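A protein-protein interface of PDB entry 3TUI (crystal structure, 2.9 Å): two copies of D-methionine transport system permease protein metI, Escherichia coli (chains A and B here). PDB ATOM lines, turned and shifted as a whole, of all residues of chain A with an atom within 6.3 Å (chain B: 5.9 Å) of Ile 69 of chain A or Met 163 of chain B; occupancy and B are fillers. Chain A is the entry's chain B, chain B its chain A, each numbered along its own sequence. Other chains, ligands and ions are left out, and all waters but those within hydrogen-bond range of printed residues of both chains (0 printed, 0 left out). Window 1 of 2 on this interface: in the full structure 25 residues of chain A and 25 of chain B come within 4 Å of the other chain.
Among the printed residues, pairs that only touch across the chains: Pro 67 of chain A with Gly 159 of chain B, Ile 69 of chain A with Ala 162 of chain B, Ile 69 of chain A with Met 163 of chain B, Ile 70 of chain A with Met 189 of chain B, Val 73 of chain A with Met 189 of chain B, Trp 74 of chain A with Met 189 of chain B, Ala 162 of chain A with Ile 69 of chain B, Met 163 of chain A with Met 163 of chain B, Ala 166 of chain A with Met 163 of chain B and Ala 166 of chain A with Ala 166 of chain B.
Of the printed residues of chain B, Pro 67 of chain A touches Gly 159 (3.7 Å). Of chain B, only Ala 162 (3.3 Å) and Met 163 (2.8 Å) come within 4 Å of Ile 69 of chain A. Printed residues of chain A within 4 Å of Ile 69 of chain B: Ala 162 (3.8 Å). Of the printed residues of chain A, Gly 159 of chain B touches Pro 67. Tyr 160 of chain B touches none of the printed residues of chain A. Met 163 of chain B touches just these residues of chain A: Ile 69, Met 163 and Ala 166. Gly 164 of chain B touches none of the printed residues of chain A. The nearest printed residue of chain B that does not touch Ile 70 of chain A is Ala 162 of chain B (4.2 Å).
Hydrophobic or aromatic side chains of chain B that line the printed part of chain A: Ile 69, Ala 162, Met 163, Ala 166 and Met 189. Along chain A the printed residues that touch a printed residue of chain B span positions 67 to 166.
Ile 69 of chain A touches Ala 162 of chain B, and with the chains exchanged Ala 162 of chain A touches Ile 69 of chain B. Ile 69 of chain A touches Met 163 of chain B, but with the chains exchanged Met 163 of chain A does not touch Ile 69 of chain B (4.3 Å). Met 163 of chain A touches its own counterpart, Met 163 of chain B. Ala 166 of chain A touches Met 163 of chain B, but with the chains exchanged Met 163 of chain A does not touch Ala 166 of chain B (6.4 Å). Of the 10 pairs that touch across the chains among the printed residues, 4 have their exchanged pair printed and touching as well.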
ATOM      1  N   ILE A  66       8.992  -0.556  17.259  1.00  0.00           N
ATOM      2  CA  ILE A  66       9.702   0.729  17.245  1.00  0.00           C
ATOM      3  C   ILE A  66       9.480   1.461  18.534  1.00  0.00           C
ATOM      4  O   ILE A  66       8.331   1.735  18.894  1.00  0.00           O
ATOM      5  CB  ILE A  66       9.225   1.637  16.127  1.00  0.00           C
ATOM      6  CG1 ILE A  66       9.248   0.884  14.799  1.00  0.00           C
ATOM      7  CG2 ILE A  66      10.068   2.856  16.098  1.00  0.00           C
ATOM      8  CD1 ILE A  66       8.404   1.519  13.725  1.00  0.00           C
ATOM      9  N   PRO A  67      10.574   1.756  19.260  1.00  0.00           N
ATOM     10  CA  PRO A  67      10.374   2.514  20.507  1.00  0.00           C
ATOM     11  C   PRO A  67       9.845   3.876  20.143  1.00  0.00           C
ATOM     12  O   PRO A  67      10.026   4.278  19.004  1.00  0.00           O
ATOM     13  CB  PRO A  67      11.779   2.599  21.111  1.00  0.00           C
ATOM     14  CG  PRO A  67      12.518   1.407  20.492  1.00  0.00           C
ATOM     15  CD  PRO A  67      11.968   1.299  19.091  1.00  0.00           C
ATOM     16  N   PHE A  68       9.177   4.563  21.053  1.00  0.00           N
ATOM     17  CA  PHE A  68       8.438   5.740  20.623  1.00  0.00           C
ATOM     18  C   PHE A  68       9.302   6.923  20.144  1.00  0.00           C
ATOM     19  O   PHE A  68       9.080   7.411  19.030  1.00  0.00           O
ATOM     20  CB  PHE A  68       7.394   6.167  21.666  1.00  0.00           C
ATOM     21  CG  PHE A  68       6.586   7.367  21.251  1.00  0.00           C
ATOM     22  CD1 PHE A  68       5.795   7.349  20.102  1.00  0.00           C
ATOM     23  CD2 PHE A  68       6.572   8.499  22.053  1.00  0.00           C
ATOM     24  CE1 PHE A  68       5.045   8.476  19.735  1.00  0.00           C
ATOM     25  CE2 PHE A  68       5.824   9.614  21.701  1.00  0.00           C
ATOM     26  CZ  PHE A  68       5.058   9.604  20.541  1.00  0.00           C
ATOM     27  N   ILE A  69      10.271   7.392  20.936  1.00  0.00           N
ATOM     28  CA  ILE A  69      11.152   8.432  20.397  1.00  0.00           C
ATOM     29  C   ILE A  69      11.780   8.100  19.070  1.00  0.00           C
ATOM     30  O   ILE A  69      11.893   8.951  18.208  1.00  0.00           O
ATOM     31  CB  ILE A  69      12.285   8.866  21.330  1.00  0.00           C
ATOM     32  CG1 ILE A  69      13.094   7.638  21.791  1.00  0.00           C
ATOM     33  CG2 ILE A  69      11.750   9.631  22.555  1.00  0.00           C
ATOM     34  CD1 ILE A  69      14.658   7.946  21.701  1.00  0.00           C
ATOM     35  N   ILE A  70      12.221   6.875  18.897  1.00  0.00           N
ATOM     36  CA  ILE A  70      12.794   6.553  17.618  1.00  0.00           C
ATOM     37  C   ILE A  70      11.736   6.726  16.536  1.00  0.00           C
ATOM     38  O   ILE A  70      12.049   7.152  15.441  1.00  0.00           O
ATOM     39  CB  ILE A  70      13.374   5.148  17.618  1.00  0.00           C
ATOM     40  CG1 ILE A  70      14.303   5.019  18.827  1.00  0.00           C
ATOM     41  CG2 ILE A  70      14.056   4.818  16.251  1.00  0.00           C
ATOM     42  CD1 ILE A  70      15.458   6.014  18.805  1.00  0.00           C
ATOM     43  N   LEU A  71      10.481   6.414  16.849  1.00  0.00           N
ATOM     44  CA  LEU A  71       9.371   6.609  15.913  1.00  0.00           C
ATOM     45  C   LEU A  71       9.023   8.074  15.714  1.00  0.00           C
ATOM     46  O   LEU A  71       8.616   8.489  14.625  1.00  0.00           O
ATOM     47  CB  LEU A  71       8.117   5.877  16.396  1.00  0.00           C
ATOM     48  CG  LEU A  71       6.957   6.046  15.412  1.00  0.00           C
ATOM     49  CD1 LEU A  71       7.114   5.106  14.207  1.00  0.00           C
ATOM     50  CD2 LEU A  71       5.623   5.841  16.139  1.00  0.00           C
ATOM     51  N   LEU A  72       9.157   8.832  16.797  1.00  0.00           N
ATOM     52  CA  LEU A  72       8.818  10.248  16.828  1.00  0.00           C
ATOM     53  C   LEU A  72       9.772  11.061  15.933  1.00  0.00           C
ATOM     54  O   LEU A  72       9.344  11.840  15.060  1.00  0.00           O
ATOM     55  CB  LEU A  72       8.868  10.726  18.281  1.00  0.00           C
ATOM     56  CG  LEU A  72       8.632  12.197  18.572  1.00  0.00           C
ATOM     57  CD1 LEU A  72       7.276  12.568  18.047  1.00  0.00           C
ATOM     58  CD2 LEU A  72       8.677  12.407  20.062  1.00  0.00           C
ATOM     59  N   VAL A  73      11.066  10.834  16.174  1.00  0.00           N
ATOM     60  CA  VAL A  73      12.179  11.374  15.404  1.00  0.00           C
ATOM     61  C   VAL A  73      12.186  10.953  13.946  1.00  0.00           C
ATOM     62  O   VAL A  73      12.305  11.786  13.047  1.00  0.00           O
ATOM     63  CB  VAL A  73      13.517  10.960  16.005  1.00  0.00           C
ATOM     64  CG1 VAL A  73      14.638  11.278  15.034  1.00  0.00           C
ATOM     65  CG2 VAL A  73      13.724  11.640  17.333  1.00  0.00           C
ATOM     66  N   TRP A  74      12.103   9.647  13.726  1.00  0.00           N
ATOM     67  CA  TRP A  74      12.149   9.089  12.395  1.00  0.00           C
ATOM     68  C   TRP A  74      10.995   9.662  11.599  1.00  0.00           C
ATOM     69  O   TRP A  74      11.075   9.777  10.376  1.00  0.00           O
ATOM     70  CB  TRP A  74      12.074   7.569  12.484  1.00  0.00           C
ATOM     71  CG  TRP A  74      11.797   6.838  11.216  1.00  0.00           C
ATOM     72  CD1 TRP A  74      12.597   6.764  10.108  1.00  0.00           C
ATOM     73  CD2 TRP A  74      10.644   6.038  10.934  1.00  0.00           C
ATOM     74  NE1 TRP A  74      12.006   5.970   9.152  1.00  0.00           N
ATOM     75  CE2 TRP A  74      10.808   5.517   9.632  1.00  0.00           C
ATOM     76  CE3 TRP A  74       9.489   5.713  11.657  1.00  0.00           C
ATOM     77  CZ2 TRP A  74       9.852   4.694   9.037  1.00  0.00           C
ATOM     78  CZ3 TRP A  74       8.549   4.892  11.068  1.00  0.00           C
ATOM     79  CH2 TRP A  74       8.732   4.394   9.767  1.00  0.00           C
ATOM     80  N   ALA A 162       5.155  13.135  27.043  1.00  0.00           N
ATOM     81  CA  ALA A 162       6.329  13.743  27.695  1.00  0.00           C
ATOM     82  C   ALA A 162       7.680  13.429  27.007  1.00  0.00           C
ATOM     83  O   ALA A 162       8.639  14.165  27.146  1.00  0.00           O
ATOM     84  CB  ALA A 162       6.393  13.354  29.166  1.00  0.00           C
ATOM     85  N   MET A 163       7.775  12.340  26.262  1.00  0.00           N
ATOM     86  CA  MET A 163       9.025  12.076  25.580  1.00  0.00           C
ATOM     87  C   MET A 163       9.180  13.123  24.511  1.00  0.00           C
ATOM     88  O   MET A 163      10.275  13.360  24.030  1.00  0.00           O
ATOM     89  CB  MET A 163       9.046  10.668  24.967  1.00  0.00           C
ATOM     90  CG  MET A 163       9.183   9.538  26.001  1.00  0.00           C
ATOM     91  SD  MET A 163       9.290   7.855  25.341  1.00  0.00           S
ATOM     92  CE  MET A 163      10.348   7.051  26.563  1.00  0.00           C
ATOM     93  N   GLY A 164       8.068  13.747  24.136  1.00  0.00           N
ATOM     94  CA  GLY A 164       8.063  14.765  23.100  1.00  0.00           C
ATOM     95  C   GLY A 164       8.727  16.084  23.477  1.00  0.00           C
ATOM     96  O   GLY A 164       9.019  16.892  22.599  1.00  0.00           O
ATOM     97  N   GLY A 165       8.967  16.311  24.772  1.00  0.00           N
ATOM     98  CA  GLY A 165       9.616  17.534  25.246  1.00  0.00           C
ATOM     99  C   GLY A 165      11.051  17.669  24.752  1.00  0.00           C
ATOM    100  O   GLY A 165      11.456  18.705  24.201  1.00  0.00           O
ATOM    101  N   ALA A 166      11.813  16.600  24.953  1.00  0.00           N
ATOM    102  CA  ALA A 166      13.117  16.456  24.339  1.00  0.00           C
ATOM    103  C   ALA A 166      13.086  16.770  22.838  1.00  0.00           C
ATOM    104  O   ALA A 166      14.012  17.386  22.322  1.00  0.00           O
ATOM    105  CB  ALA A 166      13.657  15.054  24.574  1.00  0.00           C
ATOM    106  N   VAL A 167      12.055  16.343  22.123  1.00  0.00           N
ATOM    107  CA  VAL A 167      11.959  16.715  20.710  1.00  0.00           C
ATOM    108  C   VAL A 167      11.083  17.935  20.469  1.00  0.00           C
ATOM    109  O   VAL A 167      10.660  18.186  19.333  1.00  0.00           O
ATOM    110  CB  VAL A 167      11.524  15.583  19.796  1.00  0.00           C
ATOM    111  CG1 VAL A 167      12.245  14.303  20.195  1.00  0.00           C
ATOM    112  CG2 VAL A 167       9.993  15.446  19.752  1.00  0.00           C
ATOM    113  N   PHE B  68       9.042   7.581  32.283  1.00  0.00           N
ATOM    114  CA  PHE B  68      10.465   7.347  32.519  1.00  0.00           C
ATOM    115  C   PHE B  68      11.339   8.560  32.330  1.00  0.00           C
ATOM    116  O   PHE B  68      12.232   8.819  33.151  1.00  0.00           O
ATOM    117  CB  PHE B  68      11.032   6.190  31.700  1.00  0.00           C
ATOM    118  CG  PHE B  68      12.504   5.974  31.931  1.00  0.00           C
ATOM    119  CD1 PHE B  68      12.953   5.505  33.175  1.00  0.00           C
ATOM    120  CD2 PHE B  68      13.438   6.197  30.916  1.00  0.00           C
ATOM    121  CE1 PHE B  68      14.314   5.287  33.417  1.00  0.00           C
ATOM    122  CE2 PHE B  68      14.802   5.977  31.149  1.00  0.00           C
ATOM    123  CZ  PHE B  68      15.238   5.522  32.404  1.00  0.00           C
ATOM    124  N   ILE B  69      11.116   9.296  31.246  1.00  0.00           N
ATOM    125  CA  ILE B  69      11.972  10.444  31.000  1.00  0.00           C
ATOM    126  C   ILE B  69      11.943  11.338  32.226  1.00  0.00           C
ATOM    127  O   ILE B  69      13.009  11.603  32.790  1.00  0.00           O
ATOM    128  CB  ILE B  69      11.663  11.180  29.684  1.00  0.00           C
ATOM    129  CG1 ILE B  69      12.864  12.077  29.355  1.00  0.00           C
ATOM    130  CG2 ILE B  69      10.323  11.928  29.743  1.00  0.00           C
ATOM    131  CD1 ILE B  69      12.680  12.923  28.152  1.00  0.00           C
ATOM    132  N   LEU B  72      13.966  10.015  34.904  1.00  0.00           N
ATOM    133  CA  LEU B  72      15.397  10.229  34.678  1.00  0.00           C
ATOM    134  C   LEU B  72      15.883  11.629  35.091  1.00  0.00           C
ATOM    135  O   LEU B  72      16.858  11.778  35.858  1.00  0.00           O
ATOM    136  CB  LEU B  72      15.748   9.972  33.206  1.00  0.00           C
ATOM    137  CG  LEU B  72      17.219   9.688  32.873  1.00  0.00           C
ATOM    138  CD1 LEU B  72      17.344   8.953  31.539  1.00  0.00           C
ATOM    139  CD2 LEU B  72      18.071  10.980  32.872  1.00  0.00           C
ATOM    140  N   VAL B 158      14.800  -1.319  26.369  1.00  0.00           N
ATOM    141  CA  VAL B 158      15.296  -0.704  25.139  1.00  0.00           C
ATOM    142  C   VAL B 158      14.701   0.681  24.885  1.00  0.00           C
ATOM    143  O   VAL B 158      15.437   1.691  24.800  1.00  0.00           O
ATOM    144  CB  VAL B 158      15.019  -1.546  23.902  1.00  0.00           C
ATOM    145  CG1 VAL B 158      15.198  -0.669  22.631  1.00  0.00           C
ATOM    146  CG2 VAL B 158      15.859  -2.820  23.902  1.00  0.00           C
ATOM    147  N   GLY B 159      13.376   0.748  24.794  1.00  0.00           N
ATOM    148  CA  GLY B 159      12.738   2.050  24.644  1.00  0.00           C
ATOM    149  C   GLY B 159      13.192   3.057  25.698  1.00  0.00           C
ATOM    150  O   GLY B 159      13.347   4.244  25.417  1.00  0.00           O
ATOM    151  N   TYR B 160      13.390   2.566  26.921  1.00  0.00           N
ATOM    152  CA  TYR B 160      13.809   3.385  28.052  1.00  0.00           C
ATOM    153  C   TYR B 160      15.225   3.904  27.870  1.00  0.00           C
ATOM    154  O   TYR B 160      15.486   5.100  28.040  1.00  0.00           O
ATOM    155  CB  TYR B 160      13.709   2.525  29.302  1.00  0.00           C
ATOM    156  CG  TYR B 160      12.373   2.619  29.994  1.00  0.00           C
ATOM    157  CD1 TYR B 160      11.226   3.031  29.293  1.00  0.00           C
ATOM    158  CD2 TYR B 160      12.261   2.338  31.356  1.00  0.00           C
ATOM    159  CE1 TYR B 160       9.994   3.135  29.930  1.00  0.00           C
ATOM    160  CE2 TYR B 160      11.034   2.430  32.010  1.00  0.00           C
ATOM    161  CZ  TYR B 160       9.906   2.829  31.295  1.00  0.00           C
ATOM    162  OH  TYR B 160       8.705   2.927  31.959  1.00  0.00           O
ATOM    163  N   SER B 161      16.128   2.987  27.515  1.00  0.00           N
ATOM    164  CA  SER B 161      17.513   3.335  27.220  1.00  0.00           C
ATOM    165  C   SER B 161      17.581   4.232  25.979  1.00  0.00           C
ATOM    166  O   SER B 161      18.373   5.171  25.935  1.00  0.00           O
ATOM    167  CB  SER B 161      18.393   2.091  27.023  1.00  0.00           C
ATOM    168  OG  SER B 161      17.990   1.309  25.909  1.00  0.00           O
ATOM    169  N   ALA B 162      16.774   3.963  24.962  1.00  0.00           N
ATOM    170  CA  ALA B 162      16.765   4.891  23.836  1.00  0.00           C
ATOM    171  C   ALA B 162      16.371   6.313  24.261  1.00  0.00           C
ATOM    172  O   ALA B 162      17.035   7.275  23.902  1.00  0.00           O
ATOM    173  CB  ALA B 162      15.858   4.403  22.719  1.00  0.00           C
ATOM    174  N   MET B 163      15.304   6.467  25.028  1.00  0.00           N
ATOM    175  CA  MET B 163      14.921   7.810  25.433  1.00  0.00           C
ATOM    176  C   MET B 163      15.993   8.418  26.345  1.00  0.00           C
ATOM    177  O   MET B 163      15.989   9.621  26.605  1.00  0.00           O
ATOM    178  CB  MET B 163      13.546   7.798  26.107  1.00  0.00           C
ATOM    179  CG  MET B 163      12.815   9.157  26.265  1.00  0.00           C
ATOM    180  SD  MET B 163      13.124  10.272  24.889  1.00  0.00           S
ATOM    181  CE  MET B 163      12.229  11.725  25.398  1.00  0.00           C
ATOM    182  N   GLY B 164      16.908   7.585  26.834  1.00  0.00           N
ATOM    183  CA  GLY B 164      18.031   8.075  27.622  1.00  0.00           C
ATOM    184  C   GLY B 164      19.081   8.811  26.795  1.00  0.00           C
ATOM    185  O   GLY B 164      19.912   9.541  27.342  1.00  0.00           O
ATOM    186  N   GLY B 165      19.043   8.619  25.474  1.00  0.00           N
ATOM    187  CA  GLY B 165      19.974   9.260  24.557  1.00  0.00           C
ATOM    188  C   GLY B 165      19.575  10.673  24.166  1.00  0.00           C
ATOM    189  O   GLY B 165      20.265  11.324  23.395  1.00  0.00           O
ATOM    190  N   ALA B 166      18.433  11.135  24.656  1.00  0.00           N
ATOM    191  CA  ALA B 166      18.118  12.547  24.576  1.00  0.00           C
ATOM    192  C   ALA B 166      18.821  13.250  25.718  1.00  0.00           C
ATOM    193  O   ALA B 166      19.232  14.389  25.586  1.00  0.00           O
ATOM    194  CB  ALA B 166      16.611  12.789  24.641  1.00  0.00           C
ATOM    195  N   VAL B 167      18.899  12.573  26.854  1.00  0.00           N
ATOM    196  CA  VAL B 167      19.570  13.074  28.056  1.00  0.00           C
ATOM    197  C   VAL B 167      20.997  12.527  28.235  1.00  0.00           C
ATOM    198  O   VAL B 167      21.506  12.460  29.362  1.00  0.00           O
ATOM    199  CB  VAL B 167      18.750  12.864  29.314  1.00  0.00           C
ATOM    200  CG1 VAL B 167      17.607  13.864  29.339  1.00  0.00           C
ATOM    201  CG2 VAL B 167      18.246  11.448  29.386  1.00  0.00           C
ATOM    202  N   GLY B 173      20.328   5.347  21.113  1.00  0.00           N
ATOM    203  CA  GLY B 173      19.317   6.363  21.329  1.00  0.00           C
ATOM    204  C   GLY B 173      19.915   7.737  21.130  1.00  0.00           C
ATOM    205  O   GLY B 173      19.294   8.652  20.572  1.00  0.00           O
ATOM    206  N   MET B 189      19.819   7.722  10.483  1.00  0.00           N
ATOM    207  CA  MET B 189      18.522   7.523  11.160  1.00  0.00           C
ATOM    208  C   MET B 189      17.924   6.162  10.844  1.00  0.00           C
ATOM    209  O   MET B 189      17.467   5.412  11.729  1.00  0.00           O
ATOM    210  CB  MET B 189      17.502   8.571  10.729  1.00  0.00           C
ATOM    211  CG  MET B 189      16.248   8.575  11.588  1.00  0.00           C
ATOM    212  SD  MET B 189      16.725   8.885  13.310  1.00  0.00           S
ATOM    213  CE  MET B 189      15.438   7.993  14.197  1.00  0.00           C
